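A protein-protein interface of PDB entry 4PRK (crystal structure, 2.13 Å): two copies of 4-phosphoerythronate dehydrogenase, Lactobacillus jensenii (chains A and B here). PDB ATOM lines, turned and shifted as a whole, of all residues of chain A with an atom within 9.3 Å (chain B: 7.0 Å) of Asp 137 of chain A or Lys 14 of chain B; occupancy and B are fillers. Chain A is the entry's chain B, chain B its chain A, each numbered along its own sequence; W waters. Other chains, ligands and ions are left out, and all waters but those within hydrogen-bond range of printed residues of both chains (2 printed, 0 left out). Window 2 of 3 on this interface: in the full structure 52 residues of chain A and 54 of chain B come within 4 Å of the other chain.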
ATOM      1  N   LYS A 120     -19.711  -6.292  23.654  1.00  0.00           N
ATOM      2  CA  LYS A 120     -20.697  -7.333  23.247  1.00  0.00           C
ATOM      3  C   LYS A 120     -21.752  -7.571  24.263  1.00  0.00           C
ATOM      4  O   LYS A 120     -22.204  -8.705  24.505  1.00  0.00           O
ATOM      5  CB  LYS A 120     -19.960  -8.624  22.914  1.00  0.00           C
ATOM      6  CG  LYS A 120     -19.008  -8.393  21.735  1.00  0.00           C
ATOM      7  CD  LYS A 120     -18.022  -9.542  21.634  1.00  0.00           C
ATOM      8  CE  LYS A 120     -17.283  -9.603  20.334  1.00  0.00           C
ATOM      9  NZ  LYS A 120     -16.343 -10.759  20.503  1.00  0.00           N
ATOM     10  N   GLU A 123     -24.843  -9.176  23.040  1.00  0.00           N
ATOM     11  CA  GLU A 123     -24.667 -10.564  22.735  1.00  0.00           C
ATOM     12  C   GLU A 123     -24.625 -11.343  24.020  1.00  0.00           C
ATOM     13  O   GLU A 123     -25.153 -12.457  24.094  1.00  0.00           O
ATOM     14  CB  GLU A 123     -23.402 -10.777  21.920  1.00  0.00           C
ATOM     15  CG  GLU A 123     -23.530 -10.121  20.574  1.00  0.00           C
ATOM     16  CD  GLU A 123     -22.239 -10.132  19.817  1.00  0.00           C
ATOM     17  OE1 GLU A 123     -21.509  -9.097  19.775  1.00  0.00           O
ATOM     18  OE2 GLU A 123     -21.918 -11.216  19.350  1.00  0.00           O
ATOM     19  N   PHE A 124     -24.049 -10.759  25.064  1.00  0.00           N
ATOM     20  CA  PHE A 124     -24.120 -11.425  26.356  1.00  0.00           C
ATOM     21  C   PHE A 124     -25.548 -11.522  26.842  1.00  0.00           C
ATOM     22  O   PHE A 124     -25.933 -12.547  27.379  1.00  0.00           O
ATOM     23  CB  PHE A 124     -23.327 -10.671  27.393  1.00  0.00           C
ATOM     24  CG  PHE A 124     -21.865 -11.073  27.457  1.00  0.00           C
ATOM     25  CD1 PHE A 124     -21.511 -12.296  27.966  1.00  0.00           C
ATOM     26  CD2 PHE A 124     -20.866 -10.189  27.042  1.00  0.00           C
ATOM     27  CE1 PHE A 124     -20.185 -12.672  28.067  1.00  0.00           C
ATOM     28  CE2 PHE A 124     -19.527 -10.544  27.139  1.00  0.00           C
ATOM     29  CZ  PHE A 124     -19.190 -11.783  27.677  1.00  0.00           C
ATOM     30  N   ASN A 127     -27.439 -14.322  24.958  1.00  0.00           N
ATOM     31  CA  ASN A 127     -26.993 -15.546  25.627  1.00  0.00           C
ATOM     32  C   ASN A 127     -27.706 -15.792  26.949  1.00  0.00           C
ATOM     33  O   ASN A 127     -28.175 -16.899  27.217  1.00  0.00           O
ATOM     34  CB  ASN A 127     -25.486 -15.497  25.923  1.00  0.00           C
ATOM     35  CG  ASN A 127     -24.661 -16.376  24.996  1.00  0.00           C
ATOM     36  OD1 ASN A 127     -25.119 -16.773  23.930  1.00  0.00           O
ATOM     37  ND2 ASN A 127     -23.423 -16.678  25.402  1.00  0.00           N
ATOM     38  N   THR A 134     -22.156 -18.122  30.516  1.00  0.00           N
ATOM     39  CA  THR A 134     -20.761 -18.469  30.447  1.00  0.00           C
ATOM     40  C   THR A 134     -19.999 -17.312  29.731  1.00  0.00           C
ATOM     41  O   THR A 134     -20.573 -16.306  29.337  1.00  0.00           O
ATOM     42  CB  THR A 134     -20.549 -19.827  29.734  1.00  0.00           C
ATOM     43  OG1 THR A 134     -20.911 -19.710  28.358  1.00  0.00           O
ATOM     44  CG2 THR A 134     -21.424 -20.940  30.382  1.00  0.00           C
ATOM     45  N   ASN A 135     -18.705 -17.504  29.586  1.00  0.00           N
ATOM     46  CA  ASN A 135     -17.824 -16.576  28.902  1.00  0.00           C
ATOM     47  C   ASN A 135     -17.177 -17.322  27.760  1.00  0.00           C
ATOM     48  O   ASN A 135     -16.021 -17.661  27.851  1.00  0.00           O
ATOM     49  CB  ASN A 135     -16.743 -16.098  29.861  1.00  0.00           C
ATOM     50  CG  ASN A 135     -17.291 -15.219  30.932  1.00  0.00           C
ATOM     51  OD1 ASN A 135     -18.493 -14.872  30.922  1.00  0.00           O
ATOM     52  ND2 ASN A 135     -16.424 -14.776  31.827  1.00  0.00           N
ATOM     53  N   PRO A 136     -17.939 -17.595  26.692  1.00  0.00           N
ATOM     54  CA  PRO A 136     -17.375 -18.264  25.527  1.00  0.00           C
ATOM     55  C   PRO A 136     -16.414 -17.350  24.771  1.00  0.00           C
ATOM     56  O   PRO A 136     -16.583 -16.120  24.755  1.00  0.00           O
ATOM     57  CB  PRO A 136     -18.605 -18.529  24.654  1.00  0.00           C
ATOM     58  CG  PRO A 136     -19.499 -17.404  24.960  1.00  0.00           C
ATOM     59  CD  PRO A 136     -19.274 -17.049  26.415  1.00  0.00           C
ATOM     60  N   ASP A 137     -15.432 -17.952  24.123  1.00  0.00           N
ATOM     61  CA  ASP A 137     -14.421 -17.191  23.447  1.00  0.00           C
ATOM     62  C   ASP A 137     -14.968 -16.264  22.367  1.00  0.00           C
ATOM     63  O   ASP A 137     -14.380 -15.214  22.102  1.00  0.00           O
ATOM     64  CB  ASP A 137     -13.403 -18.127  22.862  1.00  0.00           C
ATOM     65  CG  ASP A 137     -12.273 -17.379  22.178  1.00  0.00           C
ATOM     66  OD1 ASP A 137     -11.316 -16.916  22.863  1.00  0.00           O
ATOM     67  OD2 ASP A 137     -12.405 -17.244  20.945  1.00  0.00           O
ATOM     68  N   SER A 138     -16.112 -16.614  21.773  1.00  0.00           N
ATOM     69  CA  SER A 138     -16.730 -15.795  20.747  1.00  0.00           C
ATOM     70  C   SER A 138     -17.222 -14.450  21.273  1.00  0.00           C
ATOM     71  O   SER A 138     -17.468 -13.533  20.458  1.00  0.00           O
ATOM     72  CB  SER A 138     -17.950 -16.524  20.162  1.00  0.00           C
ATOM     73  OG  SER A 138     -18.990 -16.631  21.149  1.00  0.00           O
ATOM     74  N   LEU A 139     -17.476 -14.365  22.601  1.00  0.00           N
ATOM     75  CA  LEU A 139     -17.783 -13.080  23.266  1.00  0.00           C
ATOM     76  C   LEU A 139     -16.584 -12.394  23.947  1.00  0.00           C
ATOM     77  O   LEU A 139     -16.774 -11.428  24.677  1.00  0.00           O
ATOM     78  CB  LEU A 139     -18.926 -13.260  24.252  1.00  0.00           C
ATOM     79  CG  LEU A 139     -20.178 -13.847  23.599  1.00  0.00           C
ATOM     80  CD1 LEU A 139     -21.379 -13.850  24.536  1.00  0.00           C
ATOM     81  CD2 LEU A 139     -20.494 -13.078  22.334  1.00  0.00           C
ATOM     82  N   ILE A 140     -15.348 -12.851  23.692  1.00  0.00           N
ATOM     83  CA  ILE A 140     -14.166 -12.101  24.179  1.00  0.00           C
ATOM     84  C   ILE A 140     -14.044 -10.710  23.552  1.00  0.00           C
ATOM     85  O   ILE A 140     -14.393 -10.476  22.408  1.00  0.00           O
ATOM     86  CB  ILE A 140     -12.891 -12.906  23.966  1.00  0.00           C
ATOM     87  CG1 ILE A 140     -11.809 -12.445  24.958  1.00  0.00           C
ATOM     88  CG2 ILE A 140     -12.451 -12.832  22.504  1.00  0.00           C
ATOM     89  CD1 ILE A 140     -10.661 -13.413  25.140  1.00  0.00           C
ATOM     90  N   SER A 141     -13.531  -9.796  24.349  1.00  0.00           N
ATOM     91  CA  SER A 141     -13.403  -8.403  23.992  1.00  0.00           C
ATOM     92  C   SER A 141     -11.951  -7.953  24.036  1.00  0.00           C
ATOM     93  O   SER A 141     -11.048  -8.760  24.069  1.00  0.00           O
ATOM     94  CB  SER A 141     -14.255  -7.537  24.916  1.00  0.00           C
ATOM     95  OG  SER A 141     -14.496  -6.283  24.349  1.00  0.00           O
ATOM     96  N   ASN A 142     -11.737  -6.652  23.978  1.00  0.00           N
ATOM     97  CA  ASN A 142     -10.413  -6.089  24.129  1.00  0.00           C
ATOM     98  C   ASN A 142     -10.486  -4.656  24.616  1.00  0.00           C
ATOM     99  O   ASN A 142     -11.533  -3.991  24.493  1.00  0.00           O
ATOM    100  CB  ASN A 142      -9.667  -6.176  22.810  1.00  0.00           C
ATOM    101  CG  ASN A 142      -8.172  -6.383  22.995  1.00  0.00           C
ATOM    102  OD1 ASN A 142      -7.680  -6.635  24.087  1.00  0.00           O
ATOM    103  ND2 ASN A 142      -7.449  -6.284  21.911  1.00  0.00           N
ATOM    104  N   SER B   9      -9.510 -22.413  29.952  1.00  0.00           N
ATOM    105  CA  SER B   9     -10.649 -21.915  29.241  1.00  0.00           C
ATOM    106  C   SER B   9     -10.391 -22.124  27.777  1.00  0.00           C
ATOM    107  O   SER B   9      -9.262 -22.327  27.356  1.00  0.00           O
ATOM    108  CB  SER B   9     -10.819 -20.414  29.463  1.00  0.00           C
ATOM    109  OG  SER B   9     -10.031 -19.668  28.559  1.00  0.00           O
ATOM    110  N   GLU B  10     -11.446 -22.019  27.002  1.00  0.00           N
ATOM    111  CA  GLU B  10     -11.363 -22.027  25.565  1.00  0.00           C
ATOM    112  C   GLU B  10     -10.450 -20.876  24.996  1.00  0.00           C
ATOM    113  O   GLU B  10      -9.640 -21.070  24.100  1.00  0.00           O
ATOM    114  CB  GLU B  10     -12.791 -21.868  25.073  1.00  0.00           C
ATOM    115  CG  GLU B  10     -12.917 -21.733  23.574  1.00  0.00           C
ATOM    116  CD  GLU B  10     -14.354 -21.636  23.118  1.00  0.00           C
ATOM    117  OE1 GLU B  10     -15.208 -21.218  23.927  1.00  0.00           O
ATOM    118  OE2 GLU B  10     -14.607 -21.964  21.929  1.00  0.00           O
ATOM    119  N   SER B  11     -10.592 -19.678  25.540  1.00  0.00           N
ATOM    120  CA  SER B  11      -9.783 -18.552  25.149  1.00  0.00           C
ATOM    121  C   SER B  11      -8.354 -18.868  25.546  1.00  0.00           C
ATOM    122  O   SER B  11      -7.430 -18.606  24.768  1.00  0.00           O
ATOM    123  CB  SER B  11     -10.320 -17.233  25.807  1.00  0.00           C
ATOM    124  OG  SER B  11     -11.631 -16.883  25.289  1.00  0.00           O
ATOM    125  N   GLU B  12      -8.139 -19.440  26.739  1.00  0.00           N
ATOM    126  CA  GLU B  12      -6.789 -19.804  27.128  1.00  0.00           C
ATOM    127  C   GLU B  12      -6.151 -20.785  26.113  1.00  0.00           C
ATOM    128  O   GLU B  12      -4.989 -20.623  25.758  1.00  0.00           O
ATOM    129  CB  GLU B  12      -6.749 -20.370  28.531  1.00  0.00           C
ATOM    130  CG  GLU B  12      -6.819 -19.337  29.649  1.00  0.00           C
ATOM    131  CD  GLU B  12      -6.864 -19.955  31.032  1.00  0.00           C
ATOM    132  OE1 GLU B  12      -7.675 -20.845  31.259  1.00  0.00           O
ATOM    133  OE2 GLU B  12      -6.083 -19.571  31.894  1.00  0.00           O
ATOM    134  N   ARG B  13      -6.923 -21.752  25.617  1.00  0.00           N
ATOM    135  CA  ARG B  13      -6.407 -22.777  24.668  1.00  0.00           C
ATOM    136  C   ARG B  13      -5.824 -22.157  23.407  1.00  0.00           C
ATOM    137  O   ARG B  13      -4.709 -22.500  22.938  1.00  0.00           O
ATOM    138  CB  ARG B  13      -7.538 -23.729  24.263  1.00  0.00           C
ATOM    139  CG  ARG B  13      -7.969 -24.677  25.378  1.00  0.00           C
ATOM    140  CD  ARG B  13      -9.151 -25.568  24.976  1.00  0.00           C
ATOM    141  NE  ARG B  13      -9.523 -26.456  26.080  1.00  0.00           N
ATOM    142  CZ  ARG B  13      -8.854 -27.556  26.428  1.00  0.00           C
ATOM    143  NH1 ARG B  13      -7.761 -27.917  25.759  1.00  0.00           N
ATOM    144  NH2 ARG B  13      -9.258 -28.294  27.459  1.00  0.00           N
ATOM    145  N   LYS B  14      -6.601 -21.222  22.886  1.00  0.00           N
ATOM    146  CA  LYS B  14      -6.231 -20.474  21.725  1.00  0.00           C
ATOM    147  C   LYS B  14      -4.918 -19.778  21.818  1.00  0.00           C
ATOM    148  O   LYS B  14      -4.312 -19.600  20.804  1.00  0.00           O
ATOM    149  CB  LYS B  14      -7.341 -19.486  21.358  1.00  0.00           C
ATOM    150  CG  LYS B  14      -8.531 -20.223  20.742  1.00  0.00           C
ATOM    151  CD  LYS B  14      -9.608 -19.281  20.234  1.00  0.00           C
ATOM    152  CE  LYS B  14     -10.427 -19.873  19.079  1.00  0.00           C
ATOM    153  NZ  LYS B  14     -11.385 -20.928  19.472  1.00  0.00           N
ATOM    154  N   LEU B  15      -4.449 -19.372  22.990  1.00  0.00           N
ATOM    155  CA  LEU B  15      -3.133 -18.659  23.085  1.00  0.00           C
ATOM    156  C   LEU B  15      -1.969 -19.606  23.257  1.00  0.00           C
ATOM    157  O   LEU B  15      -0.826 -19.196  23.247  1.00  0.00           O
ATOM    158  CB  LEU B  15      -3.089 -17.725  24.289  1.00  0.00           C
ATOM    159  CG  LEU B  15      -4.194 -16.679  24.387  1.00  0.00           C
ATOM    160  CD1 LEU B  15      -4.046 -15.912  25.687  1.00  0.00           C
ATOM    161  CD2 LEU B  15      -4.141 -15.749  23.179  1.00  0.00           C
ATOM    162  N   VAL B  16      -2.255 -20.867  23.485  1.00  0.00           N
ATOM    163  CA  VAL B  16      -1.229 -21.742  24.003  1.00  0.00           C
ATOM    164  C   VAL B  16       0.033 -21.793  23.165  1.00  0.00           C
ATOM    165  O   VAL B  16       1.153 -21.745  23.664  1.00  0.00           O
ATOM    166  CB  VAL B  16      -1.774 -23.158  24.117  1.00  0.00           C
ATOM    167  CG1 VAL B  16      -0.623 -24.151  24.177  1.00  0.00           C
ATOM    168  CG2 VAL B  16      -2.631 -23.237  25.354  1.00  0.00           C
ATOM    169  N   ALA B  17      -0.164 -21.949  21.885  1.00  0.00           N
ATOM    170  CA  ALA B  17       0.962 -22.190  21.022  1.00  0.00           C
ATOM    171  C   ALA B  17       1.799 -20.950  21.011  1.00  0.00           C
ATOM    172  O   ALA B  17       3.008 -21.032  21.001  1.00  0.00           O
ATOM    173  CB  ALA B  17       0.479 -22.535  19.633  1.00  0.00           C
ATOM    174  N   ALA B  18       1.172 -19.782  21.001  1.00  0.00           N
ATOM    175  CA  ALA B  18       1.954 -18.537  20.928  1.00  0.00           C
ATOM    176  C   ALA B  18       2.757 -18.360  22.220  1.00  0.00           C
ATOM    177  O   ALA B  18       3.864 -17.821  22.210  1.00  0.00           O
ATOM    178  CB  ALA B  18       1.050 -17.342  20.707  1.00  0.00           C
ATOM    179  N   LEU B  29      -1.514 -29.319  28.769  1.00  0.00           N
ATOM    180  CA  LEU B  29      -2.845 -28.898  29.176  1.00  0.00           C
ATOM    181  C   LEU B  29      -3.641 -30.010  29.710  1.00  0.00           C
ATOM    182  O   LEU B  29      -3.853 -30.935  29.006  1.00  0.00           O
ATOM    183  CB  LEU B  29      -3.618 -28.319  28.015  1.00  0.00           C
ATOM    184  CG  LEU B  29      -3.293 -26.840  27.868  1.00  0.00           C
ATOM    185  CD1 LEU B  29      -1.807 -26.566  27.629  1.00  0.00           C
ATOM    186  CD2 LEU B  29      -4.170 -26.315  26.748  1.00  0.00           C
ATOM    187  N   PHE B 299     -13.054  -9.822  30.740  1.00  0.00           N
ATOM    188  CA  PHE B 299     -12.877 -10.827  29.688  1.00  0.00           C
ATOM    189  C   PHE B 299     -12.419 -10.165  28.378  1.00  0.00           C
ATOM    190  O   PHE B 299     -13.253  -9.952  27.438  1.00  0.00           O
ATOM    191  CB  PHE B 299     -14.207 -11.601  29.532  1.00  0.00           C
ATOM    192  CG  PHE B 299     -14.153 -12.772  28.585  1.00  0.00           C
ATOM    193  CD1 PHE B 299     -13.071 -13.644  28.576  1.00  0.00           C
ATOM    194  CD2 PHE B 299     -15.223 -13.042  27.755  1.00  0.00           C
ATOM    195  CE1 PHE B 299     -13.039 -14.708  27.695  1.00  0.00           C
ATOM    196  CE2 PHE B 299     -15.202 -14.120  26.891  1.00  0.00           C
ATOM    197  CZ  PHE B 299     -14.107 -14.960  26.880  1.00  0.00           C
ATOM    198  N   LYS B 301      -8.723 -10.111  25.626  1.00  0.00           N
ATOM    199  CA  LYS B 301      -7.566 -10.887  25.203  1.00  0.00           C
ATOM    200  C   LYS B 301      -6.382 -10.606  26.112  1.00  0.00           C
ATOM    201  O   LYS B 301      -5.644 -11.481  26.454  1.00  0.00           O
ATOM    202  CB  LYS B 301      -7.136 -10.467  23.812  1.00  0.00           C
ATOM    203  CG  LYS B 301      -8.178 -10.654  22.721  1.00  0.00           C
ATOM    204  CD  LYS B 301      -8.051 -12.007  22.057  1.00  0.00           C
ATOM    205  CE  LYS B 301      -8.747 -12.018  20.706  1.00  0.00           C
ATOM    206  NZ  LYS B 301      -8.492 -13.356  20.084  1.00  0.00           N
ATOM    207  N   VAL B 304      -6.886 -12.561  29.539  1.00  0.00           N
ATOM    208  CA  VAL B 304      -6.766 -14.005  29.445  1.00  0.00           C
ATOM    209  C   VAL B 304      -5.276 -14.349  29.221  1.00  0.00           C
ATOM    210  O   VAL B 304      -4.739 -15.225  29.872  1.00  0.00           O
ATOM    211  CB  VAL B 304      -7.676 -14.553  28.346  1.00  0.00           C
ATOM    212  CG1 VAL B 304      -7.363 -16.027  28.022  1.00  0.00           C
ATOM    213  CG2 VAL B 304      -9.111 -14.394  28.782  1.00  0.00           C
HETATM  214  O   HOH W   1     -15.864  -9.957  26.837  1.00  0.00           O
HETATM  215  O   HOH W   2      -8.951 -15.547  22.185  1.00  0.00           O
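No position is printed for both chains. Of the 13 pairs that touch across the chains among the printed residues, none has its exchanged pair printed and touching as well.
Of chain B, only Glu 10, Ser 11 and Lys 14 come within 4 Å of Asp 137 of chain A. Of chain A, only Asp 137 comes within 4 Å of Lys 14 of chain B. Ser 11 of chain B touches just these residues of chain A: Asp 137 and Ile 140. Of the printed residues of chain B, Asn 135 of chain A touches Phe 299 (3.4 Å). Of the printed residues of chain B, Pro 136 of chain A touches Glu 10 (3.998 Å) and Phe 299 (3.2 Å). Of the printed residues of chain B, Ile 140 of chain A touches Ser 11 (3.6 Å), Phe 299 (3.4 Å) and Lys 301 (3.9 Å). Ala 17 of chain B touches none of the printed residues of chain A. The nearest residue of chain A that does not touch Lys 14 of chain B is Ser 138 of chain A (6.8 Å).
Printed residues of chain B that touch a printed residue of chain A: Glu 10, Ser 11, Lys 14, Phe 299 and Lys 301. Hydrophobic or aromatic side chains of chain B that line the printed part of chain A: Phe 299. Hydrophobic or aromatic side chains of chain A that line the printed part of chain B: Ile 140. Among the printed residues, no Asp or Glu carboxylate lies within 4 Å of a Lys or Arg side-chain nitrogen of the other chain.
Among the printed residues, merely in contact across the chains: Pro 136 of chain A with Phe 299 of chain B, Ile 140 of chain A with Phe 299 of chain B, Asn 135 of chain A with Phe 299 of chain B, Asp 137 of chain A with Lys 14 of chain B, Ile 140 of chain A with Ser 11 of chain B, Leu 139 of chain A with Phe 299 of chain B, Ile 140 of chain A with Lys 301 of chain B, Asn 142 of chain A with Lys 301 of chain B and Pro 136 of chain A with Glu 10 of chain B.
N of Asp 137 of chain A is in hydrogen-bond range of OE1 of Glu 10 of chain B, 3.3 Å away. The side-chain hydroxyl (OG) of Ser 11 of chain B sits at hydrogen-bond distance from the side-chain carboxylate (OD1) of Asp 137 of chain A. The backbone carbonyl oxygen (O) of Phe 299 of chain B sits at hydrogen-bond distance from the backbone NH (N) of Ser 141 of chain A (3.1 Å). O of Ser 141 of chain A sits at hydrogen-bond distance from N of Lys 301 of chain B (3.1 Å).
Water W1 lies within hydrogen-bond range of the backbone carbonyl oxygen (O) of Phe 299 of chain B, the backbone carbonyl oxygen (O) of Leu 139 of chain A and the backbone NH (N) of Ser 141 of chain A. Water W2 lies within hydrogen-bond range of OD1 of Asp 137 of chain A and NZ of Lys 301 of chain B.
OG of Ser 9 of chain B is in hydrogen-bond range of N of Ser 11 of chain B (3.1 Å). The side-chain amino group of Lys 120 of chain A lies within hydrogen-bond range of the backbone carbonyl oxygen of Ile 140 of chain A (2.7 Å).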
